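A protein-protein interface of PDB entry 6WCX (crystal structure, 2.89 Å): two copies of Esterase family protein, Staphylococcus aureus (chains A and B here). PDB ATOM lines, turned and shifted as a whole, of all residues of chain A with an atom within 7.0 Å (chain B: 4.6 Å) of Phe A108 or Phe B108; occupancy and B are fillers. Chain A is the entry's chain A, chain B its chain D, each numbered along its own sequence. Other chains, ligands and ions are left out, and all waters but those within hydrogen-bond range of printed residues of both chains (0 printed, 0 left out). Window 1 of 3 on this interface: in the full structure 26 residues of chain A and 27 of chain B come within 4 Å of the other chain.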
ATOM      1  N   ILE A   6       2.568  12.592  34.729  1.00  0.00           N
ATOM      2  CA  ILE A   6       2.861  12.621  33.304  1.00  0.00           C
ATOM      3  C   ILE A   6       4.327  12.267  33.104  1.00  0.00           C
ATOM      4  O   ILE A   6       5.209  12.891  33.707  1.00  0.00           O
ATOM      5  CB  ILE A   6       2.533  14.000  32.701  1.00  0.00           C
ATOM      6  CG1 ILE A   6       1.063  14.364  32.967  1.00  0.00           C
ATOM      7  CG2 ILE A   6       2.847  14.008  31.229  1.00  0.00           C
ATOM      8  CD1 ILE A   6       0.575  15.594  32.267  1.00  0.00           C
ATOM      9  N   SER A   7       4.584  11.261  32.270  1.00  0.00           N
ATOM     10  CA  SER A   7       5.939  10.854  31.913  1.00  0.00           C
ATOM     11  C   SER A   7       6.118  11.000  30.406  1.00  0.00           C
ATOM     12  O   SER A   7       5.368  10.403  29.629  1.00  0.00           O
ATOM     13  CB  SER A   7       6.221   9.427  32.389  1.00  0.00           C
ATOM     14  OG  SER A   7       5.783   8.475  31.445  1.00  0.00           O
ATOM     15  N   LEU A   8       7.091  11.800  29.995  1.00  0.00           N
ATOM     16  CA  LEU A   8       7.345  12.071  28.592  1.00  0.00           C
ATOM     17  C   LEU A   8       8.629  11.385  28.152  1.00  0.00           C
ATOM     18  O   LEU A   8       9.576  11.263  28.932  1.00  0.00           O
ATOM     19  CB  LEU A   8       7.480  13.572  28.337  1.00  0.00           C
ATOM     20  CG  LEU A   8       6.225  14.427  28.261  1.00  0.00           C
ATOM     21  CD1 LEU A   8       5.998  15.080  29.589  1.00  0.00           C
ATOM     22  CD2 LEU A   8       6.386  15.468  27.174  1.00  0.00           C
ATOM     23  N   LEU A  21      11.391  12.021  30.948  1.00  0.00           N
ATOM     24  CA  LEU A  21      11.094  13.217  31.717  1.00  0.00           C
ATOM     25  C   LEU A  21       9.780  12.975  32.443  1.00  0.00           C
ATOM     26  O   LEU A  21       8.862  12.374  31.882  1.00  0.00           O
ATOM     27  CB  LEU A  21      11.024  14.429  30.792  1.00  0.00           C
ATOM     28  CG  LEU A  21      10.347  15.693  31.282  1.00  0.00           C
ATOM     29  CD1 LEU A  21      11.186  16.362  32.320  1.00  0.00           C
ATOM     30  CD2 LEU A  21      10.119  16.624  30.102  1.00  0.00           C
ATOM     31  N   VAL A  23       6.587  14.637  34.888  1.00  0.00           N
ATOM     32  CA  VAL A  23       5.836  15.873  35.103  1.00  0.00           C
ATOM     33  C   VAL A  23       4.687  15.587  36.057  1.00  0.00           C
ATOM     34  O   VAL A  23       3.899  14.667  35.824  1.00  0.00           O
ATOM     35  CB  VAL A  23       5.291  16.470  33.783  1.00  0.00           C
ATOM     36  CG1 VAL A  23       4.522  17.749  34.059  1.00  0.00           C
ATOM     37  CG2 VAL A  23       6.417  16.793  32.810  1.00  0.00           C
ATOM     38  N   LEU A  25       1.331  17.380  37.100  1.00  0.00           N
ATOM     39  CA  LEU A  25       0.432  18.433  36.637  1.00  0.00           C
ATOM     40  C   LEU A  25      -0.831  18.375  37.479  1.00  0.00           C
ATOM     41  O   LEU A  25      -1.721  17.551  37.195  1.00  0.00           O
ATOM     42  CB  LEU A  25       0.101  18.273  35.163  1.00  0.00           C
ATOM     43  CG  LEU A  25      -0.210  19.570  34.426  1.00  0.00           C
ATOM     44  CD1 LEU A  25       1.063  20.337  34.143  1.00  0.00           C
ATOM     45  CD2 LEU A  25      -0.954  19.285  33.131  1.00  0.00           C
ATOM     46  N   PRO A  40      -2.870  29.257  33.759  1.00  0.00           N
ATOM     47  CA  PRO A  40      -1.600  28.525  33.846  1.00  0.00           C
ATOM     48  C   PRO A  40      -1.125  28.347  35.284  1.00  0.00           C
ATOM     49  O   PRO A  40      -1.310  29.219  36.137  1.00  0.00           O
ATOM     50  CB  PRO A  40      -0.628  29.406  33.043  1.00  0.00           C
ATOM     51  CG  PRO A  40      -1.502  30.365  32.263  1.00  0.00           C
ATOM     52  CD  PRO A  40      -2.704  30.576  33.131  1.00  0.00           C
ATOM     53  N   ILE A  75       8.442  19.630  37.485  1.00  0.00           N
ATOM     54  CA  ILE A  75       9.169  19.139  36.318  1.00  0.00           C
ATOM     55  C   ILE A  75      10.434  18.434  36.801  1.00  0.00           C
ATOM     56  O   ILE A  75      11.346  19.078  37.350  1.00  0.00           O
ATOM     57  CB  ILE A  75       9.529  20.286  35.356  1.00  0.00           C
ATOM     58  CG1 ILE A  75       8.356  21.235  35.128  1.00  0.00           C
ATOM     59  CG2 ILE A  75      10.002  19.749  34.012  1.00  0.00           C
ATOM     60  CD1 ILE A  75       7.056  20.583  34.631  1.00  0.00           C
ATOM     61  N   TYR A 103      10.445  23.597  26.604  1.00  0.00           N
ATOM     62  CA  TYR A 103       9.542  22.602  26.029  1.00  0.00           C
ATOM     63  C   TYR A 103       8.245  22.485  26.828  1.00  0.00           C
ATOM     64  O   TYR A 103       7.152  22.481  26.252  1.00  0.00           O
ATOM     65  CB  TYR A 103      10.251  21.256  25.963  1.00  0.00           C
ATOM     66  CG  TYR A 103       9.459  20.152  25.330  1.00  0.00           C
ATOM     67  CD1 TYR A 103       9.269  20.102  23.958  1.00  0.00           C
ATOM     68  CD2 TYR A 103       8.899  19.153  26.107  1.00  0.00           C
ATOM     69  CE1 TYR A 103       8.544  19.068  23.378  1.00  0.00           C
ATOM     70  CE2 TYR A 103       8.177  18.135  25.545  1.00  0.00           C
ATOM     71  CZ  TYR A 103       8.000  18.088  24.188  1.00  0.00           C
ATOM     72  OH  TYR A 103       7.273  17.052  23.647  1.00  0.00           O
ATOM     73  N   VAL A 104       8.344  22.376  28.156  1.00  0.00           N
ATOM     74  CA  VAL A 104       7.138  22.185  28.960  1.00  0.00           C
ATOM     75  C   VAL A 104       6.344  23.474  29.145  1.00  0.00           C
ATOM     76  O   VAL A 104       5.149  23.412  29.454  1.00  0.00           O
ATOM     77  CB  VAL A 104       7.465  21.544  30.319  1.00  0.00           C
ATOM     78  CG1 VAL A 104       8.099  20.181  30.101  1.00  0.00           C
ATOM     79  CG2 VAL A 104       8.354  22.446  31.168  1.00  0.00           C
ATOM     80  N   HIS A 105       6.961  24.647  28.987  1.00  0.00           N
ATOM     81  CA  HIS A 105       6.158  25.860  29.045  1.00  0.00           C
ATOM     82  C   HIS A 105       5.369  26.059  27.756  1.00  0.00           C
ATOM     83  O   HIS A 105       4.278  26.644  27.786  1.00  0.00           O
ATOM     84  CB  HIS A 105       7.045  27.065  29.354  1.00  0.00           C
ATOM     85  CG  HIS A 105       7.365  27.210  30.812  1.00  0.00           C
ATOM     86  ND1 HIS A 105       8.331  26.453  31.443  1.00  0.00           N
ATOM     87  CD2 HIS A 105       6.837  28.015  31.766  1.00  0.00           C
ATOM     88  CE1 HIS A 105       8.388  26.789  32.721  1.00  0.00           C
ATOM     89  NE2 HIS A 105       7.490  27.732  32.944  1.00  0.00           N
ATOM     90  N   GLN A 106       5.865  25.524  26.635  1.00  0.00           N
ATOM     91  CA  GLN A 106       5.143  25.632  25.371  1.00  0.00           C
ATOM     92  C   GLN A 106       4.016  24.603  25.257  1.00  0.00           C
ATOM     93  O   GLN A 106       2.953  24.911  24.706  1.00  0.00           O
ATOM     94  CB  GLN A 106       6.106  25.478  24.192  1.00  0.00           C
ATOM     95  CG  GLN A 106       7.106  26.599  24.010  1.00  0.00           C
ATOM     96  CD  GLN A 106       6.489  27.885  23.527  1.00  0.00           C
ATOM     97  OE1 GLN A 106       6.159  28.765  24.327  1.00  0.00           O
ATOM     98  NE2 GLN A 106       6.346  28.020  22.209  1.00  0.00           N
ATOM     99  N   ILE A 107       4.232  23.364  25.711  1.00  0.00           N
ATOM    100  CA  ILE A 107       3.251  22.311  25.480  1.00  0.00           C
ATOM    101  C   ILE A 107       2.358  22.026  26.683  1.00  0.00           C
ATOM    102  O   ILE A 107       1.327  21.352  26.523  1.00  0.00           O
ATOM    103  CB  ILE A 107       3.915  20.993  25.020  1.00  0.00           C
ATOM    104  CG1 ILE A 107       4.524  20.239  26.196  1.00  0.00           C
ATOM    105  CG2 ILE A 107       4.954  21.244  23.958  1.00  0.00           C
ATOM    106  CD1 ILE A 107       4.473  18.744  26.024  1.00  0.00           C
ATOM    107  N   PHE A 108       2.691  22.529  27.867  1.00  0.00           N
ATOM    108  CA  PHE A 108       1.825  22.316  29.018  1.00  0.00           C
ATOM    109  C   PHE A 108       1.277  23.651  29.512  1.00  0.00           C
ATOM    110  O   PHE A 108       1.891  24.701  29.274  1.00  0.00           O
ATOM    111  CB  PHE A 108       2.591  21.615  30.152  1.00  0.00           C
ATOM    112  CG  PHE A 108       2.753  20.144  29.958  1.00  0.00           C
ATOM    113  CD1 PHE A 108       1.650  19.313  29.918  1.00  0.00           C
ATOM    114  CD2 PHE A 108       4.012  19.591  29.831  1.00  0.00           C
ATOM    115  CE1 PHE A 108       1.800  17.955  29.750  1.00  0.00           C
ATOM    116  CE2 PHE A 108       4.172  18.228  29.659  1.00  0.00           C
ATOM    117  CZ  PHE A 108       3.065  17.409  29.621  1.00  0.00           C
ATOM    118  N   PRO A 109       0.114  23.661  30.174  1.00  0.00           N
ATOM    119  CA  PRO A 109      -0.413  24.927  30.699  1.00  0.00           C
ATOM    120  C   PRO A 109       0.366  25.449  31.899  1.00  0.00           C
ATOM    121  O   PRO A 109      -0.119  25.421  33.037  1.00  0.00           O
ATOM    122  CB  PRO A 109      -1.844  24.562  31.093  1.00  0.00           C
ATOM    123  CG  PRO A 109      -1.785  23.129  31.405  1.00  0.00           C
ATOM    124  CD  PRO A 109      -0.832  22.556  30.410  1.00  0.00           C
ATOM    125  N   LEU A 110       1.576  25.932  31.666  1.00  0.00           N
ATOM    126  CA  LEU A 110       2.418  26.420  32.738  1.00  0.00           C
ATOM    127  C   LEU A 110       2.590  27.924  32.592  1.00  0.00           C
ATOM    128  O   LEU A 110       2.672  28.439  31.472  1.00  0.00           O
ATOM    129  CB  LEU A 110       3.769  25.701  32.731  1.00  0.00           C
ATOM    130  CG  LEU A 110       3.680  24.174  32.695  1.00  0.00           C
ATOM    131  CD1 LEU A 110       5.057  23.516  32.760  1.00  0.00           C
ATOM    132  CD2 LEU A 110       2.798  23.667  33.825  1.00  0.00           C
ATOM    133  N   SER A 111       2.592  28.621  33.732  1.00  0.00           N
ATOM    134  CA  SER A 111       2.887  30.050  33.768  1.00  0.00           C
ATOM    135  C   SER A 111       4.299  30.344  33.293  1.00  0.00           C
ATOM    136  O   SER A 111       5.266  29.744  33.772  1.00  0.00           O
ATOM    137  CB  SER A 111       2.693  30.589  35.179  1.00  0.00           C
ATOM    138  OG  SER A 111       2.852  31.999  35.232  1.00  0.00           O
ATOM    139  N   LYS A 112       4.423  31.298  32.378  1.00  0.00           N
ATOM    140  CA  LYS A 112       5.740  31.760  31.972  1.00  0.00           C
ATOM    141  C   LYS A 112       6.215  32.982  32.753  1.00  0.00           C
ATOM    142  O   LYS A 112       7.296  33.501  32.455  1.00  0.00           O
ATOM    143  CB  LYS A 112       5.741  32.053  30.472  1.00  0.00           C
ATOM    144  CG  LYS A 112       5.246  30.883  29.632  1.00  0.00           C
ATOM    145  CD  LYS A 112       5.616  31.041  28.170  1.00  0.00           C
ATOM    146  CE  LYS A 112       4.680  30.238  27.295  1.00  0.00           C
ATOM    147  NZ  LYS A 112       3.684  31.151  26.651  1.00  0.00           N
ATOM    148  N   ILE B   6       3.824  10.086  25.409  1.00  0.00           N
ATOM    149  CA  ILE B   6       3.413  10.643  26.689  1.00  0.00           C
ATOM    150  C   ILE B   6       2.406   9.697  27.317  1.00  0.00           C
ATOM    151  O   ILE B   6       1.439   9.293  26.663  1.00  0.00           O
ATOM    152  CB  ILE B   6       2.816  12.052  26.519  1.00  0.00           C
ATOM    153  CG1 ILE B   6       3.819  12.987  25.844  1.00  0.00           C
ATOM    154  CG2 ILE B   6       2.406  12.630  27.842  1.00  0.00           C
ATOM    155  CD1 ILE B   6       3.245  14.345  25.543  1.00  0.00           C
ATOM    156  N   LEU B   8      -0.083   9.479  30.587  1.00  0.00           N
ATOM    157  CA  LEU B   8      -0.770  10.267  31.596  1.00  0.00           C
ATOM    158  C   LEU B   8      -1.556   9.360  32.533  1.00  0.00           C
ATOM    159  O   LEU B   8      -2.063   8.312  32.125  1.00  0.00           O
ATOM    160  CB  LEU B   8      -1.743  11.257  30.960  1.00  0.00           C
ATOM    161  CG  LEU B   8      -1.194  12.401  30.127  1.00  0.00           C
ATOM    162  CD1 LEU B   8      -1.204  12.037  28.670  1.00  0.00           C
ATOM    163  CD2 LEU B   8      -2.022  13.642  30.355  1.00  0.00           C
ATOM    164  N   VAL B  23      -0.643   9.381  24.926  1.00  0.00           N
ATOM    165  CA  VAL B  23      -0.735  10.442  23.934  1.00  0.00           C
ATOM    166  C   VAL B  23       0.552  10.423  23.125  1.00  0.00           C
ATOM    167  O   VAL B  23       1.644  10.404  23.701  1.00  0.00           O
ATOM    168  CB  VAL B  23      -0.947  11.820  24.604  1.00  0.00           C
ATOM    169  CG1 VAL B  23      -0.667  12.966  23.639  1.00  0.00           C
ATOM    170  CG2 VAL B  23      -2.350  11.938  25.163  1.00  0.00           C
ATOM    171  N   LEU B  25       2.645  12.801  20.781  1.00  0.00           N
ATOM    172  CA  LEU B  25       2.758  14.225  20.489  1.00  0.00           C
ATOM    173  C   LEU B  25       3.969  14.398  19.583  1.00  0.00           C
ATOM    174  O   LEU B  25       5.114  14.302  20.057  1.00  0.00           O
ATOM    175  CB  LEU B  25       2.884  15.025  21.775  1.00  0.00           C
ATOM    176  CG  LEU B  25       2.517  16.498  21.705  1.00  0.00           C
ATOM    177  CD1 LEU B  25       1.074  16.619  21.324  1.00  0.00           C
ATOM    178  CD2 LEU B  25       2.786  17.168  23.052  1.00  0.00           C
ATOM    179  N   VAL B 104      -7.264  17.058  26.929  1.00  0.00           N
ATOM    180  CA  VAL B 104      -6.013  17.130  26.180  1.00  0.00           C
ATOM    181  C   VAL B 104      -6.015  18.298  25.203  1.00  0.00           C
ATOM    182  O   VAL B 104      -4.946  18.758  24.798  1.00  0.00           O
ATOM    183  CB  VAL B 104      -5.719  15.799  25.451  1.00  0.00           C
ATOM    184  CG1 VAL B 104      -5.688  14.654  26.443  1.00  0.00           C
ATOM    185  CG2 VAL B 104      -6.739  15.518  24.366  1.00  0.00           C
ATOM    186  N   HIS B 105      -7.192  18.812  24.830  1.00  0.00           N
ATOM    187  CA  HIS B 105      -7.238  20.047  24.057  1.00  0.00           C
ATOM    188  C   HIS B 105      -6.986  21.260  24.938  1.00  0.00           C
ATOM    189  O   HIS B 105      -6.518  22.288  24.443  1.00  0.00           O
ATOM    190  CB  HIS B 105      -8.584  20.178  23.356  1.00  0.00           C
ATOM    191  CG  HIS B 105      -8.708  19.333  22.130  1.00  0.00           C
ATOM    192  ND1 HIS B 105      -8.841  17.963  22.182  1.00  0.00           N
ATOM    193  CD2 HIS B 105      -8.745  19.663  20.816  1.00  0.00           C
ATOM    194  CE1 HIS B 105      -8.945  17.484  20.954  1.00  0.00           C
ATOM    195  NE2 HIS B 105      -8.892  18.495  20.107  1.00  0.00           N
ATOM    196  N   GLN B 106      -7.276  21.155  26.238  1.00  0.00           N
ATOM    197  CA  GLN B 106      -6.981  22.249  27.160  1.00  0.00           C
ATOM    198  C   GLN B 106      -5.521  22.233  27.591  1.00  0.00           C
ATOM    199  O   GLN B 106      -4.948  23.295  27.845  1.00  0.00           O
ATOM    200  CB  GLN B 106      -7.896  22.208  28.390  1.00  0.00           C
ATOM    201  CG  GLN B 106      -9.369  22.532  28.145  1.00  0.00           C
ATOM    202  CD  GLN B 106      -9.648  23.973  27.777  1.00  0.00           C
ATOM    203  OE1 GLN B 106      -9.579  24.342  26.610  1.00  0.00           O
ATOM    204  NE2 GLN B 106     -10.020  24.784  28.764  1.00  0.00           N
ATOM    205  N   ILE B 107      -4.919  21.055  27.752  1.00  0.00           N
ATOM    206  CA  ILE B 107      -3.563  20.998  28.289  1.00  0.00           C
ATOM    207  C   ILE B 107      -2.453  20.790  27.242  1.00  0.00           C
ATOM    208  O   ILE B 107      -1.309  21.199  27.490  1.00  0.00           O
ATOM    209  CB  ILE B 107      -3.466  19.930  29.401  1.00  0.00           C
ATOM    210  CG1 ILE B 107      -3.526  18.509  28.842  1.00  0.00           C
ATOM    211  CG2 ILE B 107      -4.564  20.125  30.413  1.00  0.00           C
ATOM    212  CD1 ILE B 107      -2.763  17.523  29.698  1.00  0.00           C
ATOM    213  N   PHE B 108      -2.754  20.212  26.079  1.00  0.00           N
ATOM    214  CA  PHE B 108      -1.743  20.005  25.048  1.00  0.00           C
ATOM    215  C   PHE B 108      -1.961  20.968  23.888  1.00  0.00           C
ATOM    216  O   PHE B 108      -3.075  21.464  23.682  1.00  0.00           O
ATOM    217  CB  PHE B 108      -1.769  18.556  24.526  1.00  0.00           C
ATOM    218  CG  PHE B 108      -1.148  17.567  25.453  1.00  0.00           C
ATOM    219  CD1 PHE B 108       0.185  17.671  25.800  1.00  0.00           C
ATOM    220  CD2 PHE B 108      -1.897  16.522  25.974  1.00  0.00           C
ATOM    221  CE1 PHE B 108       0.767  16.751  26.659  1.00  0.00           C
ATOM    222  CE2 PHE B 108      -1.323  15.601  26.833  1.00  0.00           C
ATOM    223  CZ  PHE B 108       0.015  15.719  27.178  1.00  0.00           C
ATOM    224  N   PRO B 109      -0.899  21.285  23.107  1.00  0.00           N
ATOM    225  CA  PRO B 109      -1.069  22.197  21.962  1.00  0.00           C
ATOM    226  C   PRO B 109      -1.823  21.590  20.789  1.00  0.00           C
ATOM    227  O   PRO B 109      -1.261  21.399  19.709  1.00  0.00           O
ATOM    228  CB  PRO B 109       0.377  22.527  21.576  1.00  0.00           C
ATOM    229  CG  PRO B 109       1.157  21.385  22.088  1.00  0.00           C
ATOM    230  CD  PRO B 109       0.525  21.028  23.367  1.00  0.00           C
ATOM    231  N   LEU B 110      -3.106  21.322  20.984  1.00  0.00           N
ATOM    232  CA  LEU B 110      -3.940  20.632  20.013  1.00  0.00           C
ATOM    233  C   LEU B 110      -4.956  21.615  19.458  1.00  0.00           C
ATOM    234  O   LEU B 110      -5.439  22.488  20.188  1.00  0.00           O
ATOM    235  CB  LEU B 110      -4.673  19.452  20.653  1.00  0.00           C
ATOM    236  CG  LEU B 110      -3.868  18.471  21.502  1.00  0.00           C
ATOM    237  CD1 LEU B 110      -4.737  17.310  21.854  1.00  0.00           C
ATOM    238  CD2 LEU B 110      -2.617  17.992  20.802  1.00  0.00           C
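O of Ile A107 sits close to O of Ile B107 (2.8 Å).
O of Ile B6 sits at hydrogen-bond distance from N of Val B23, at 2.7 Å. The backbone carbonyl oxygen (O) of Ile A6 lies within hydrogen-bond range of the backbone NH (N) of Val A23. The backbone NH (N) of Leu A8 lies within hydrogen-bond range of the backbone carbonyl oxygen (O) of Leu A21 (2.7 Å).
Among the printed residues, merely in contact across the chains: Pro A109 with Ile B107 (3.3 Å), Ile A107 with Pro B109 (3.3 Å), Phe A108 with Phe B108 (3.5 Å), Ser A7 with Ile B6 (3.5 Å), Phe A108 with Ile B107 (3.7 Å), Ile A107 with Phe B108 (3.7 Å), Ile A6 with Ile B6 (3.7 Å), Leu A8 with Ile B6 (3.7 Å), Ile A107 with Leu B25 (3.8 Å) and Ile A6 with Leu B8 (3.8 Å).
Printed residues of chain B within 4 Å of Ile A107: Leu B25 (3.8 Å), Ile B107 (2.8 Å), Phe B108 (3.7 Å) and Pro B109 (3.3 Å). Ser A111 touches none of the printed residues of chain B. Of the printed residues of chain A, Leu B8 touches Ile A6 (3.8 Å). Val B23 touches none of the printed residues of chain A. Of chain A, only Ile A107 (3.7 Å) and Phe A108 (3.5 Å) come within 4 Å of Phe B108. Printed residues of chain A within 4 Å of Pro B109: Ile A107 (3.3 Å). The nearest printed residue of chain B that does not touch Phe A108 is Ile B6 (5.1 Å). The nearest printed residue of chain B that does not touch Pro A109 is Gln B106 (4.7 Å).
Of the 18 printed residues of chain A, 6 touch a printed residue of chain B. Hydrophobic or aromatic side chains of chain A within 4 Å of the printed part of chain B: Ile A6, Leu A8, Ile A107, Phe A108 and Pro A109. Of the 11 printed residues of chain B, 6 touch a printed residue of chain A. Hydrophobic or aromatic side chains of chain B within 4 Å of the printed part of chain A: Ile B6, Leu B8, Leu B25, Ile B107, Phe B108 and Pro B109. Among the printed residues, 11 pairs touch across the chains. Among the printed residues, no Asp or Glu carboxylate lies within 4 Å of a Lys or Arg side-chain nitrogen of the other chain.
Ile A107 touches Leu B25, but with the chains exchanged Leu A25 does not touch Ile B107 (4.3 Å). Ile B107 touches its own counterpart, Ile A107. Ile A107 touches Phe B108, and with the chains exchanged Phe A108 touches Ile B107. Ile A107 touches Pro B109, and with the chains exchanged Pro A109 touches Ile B107.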
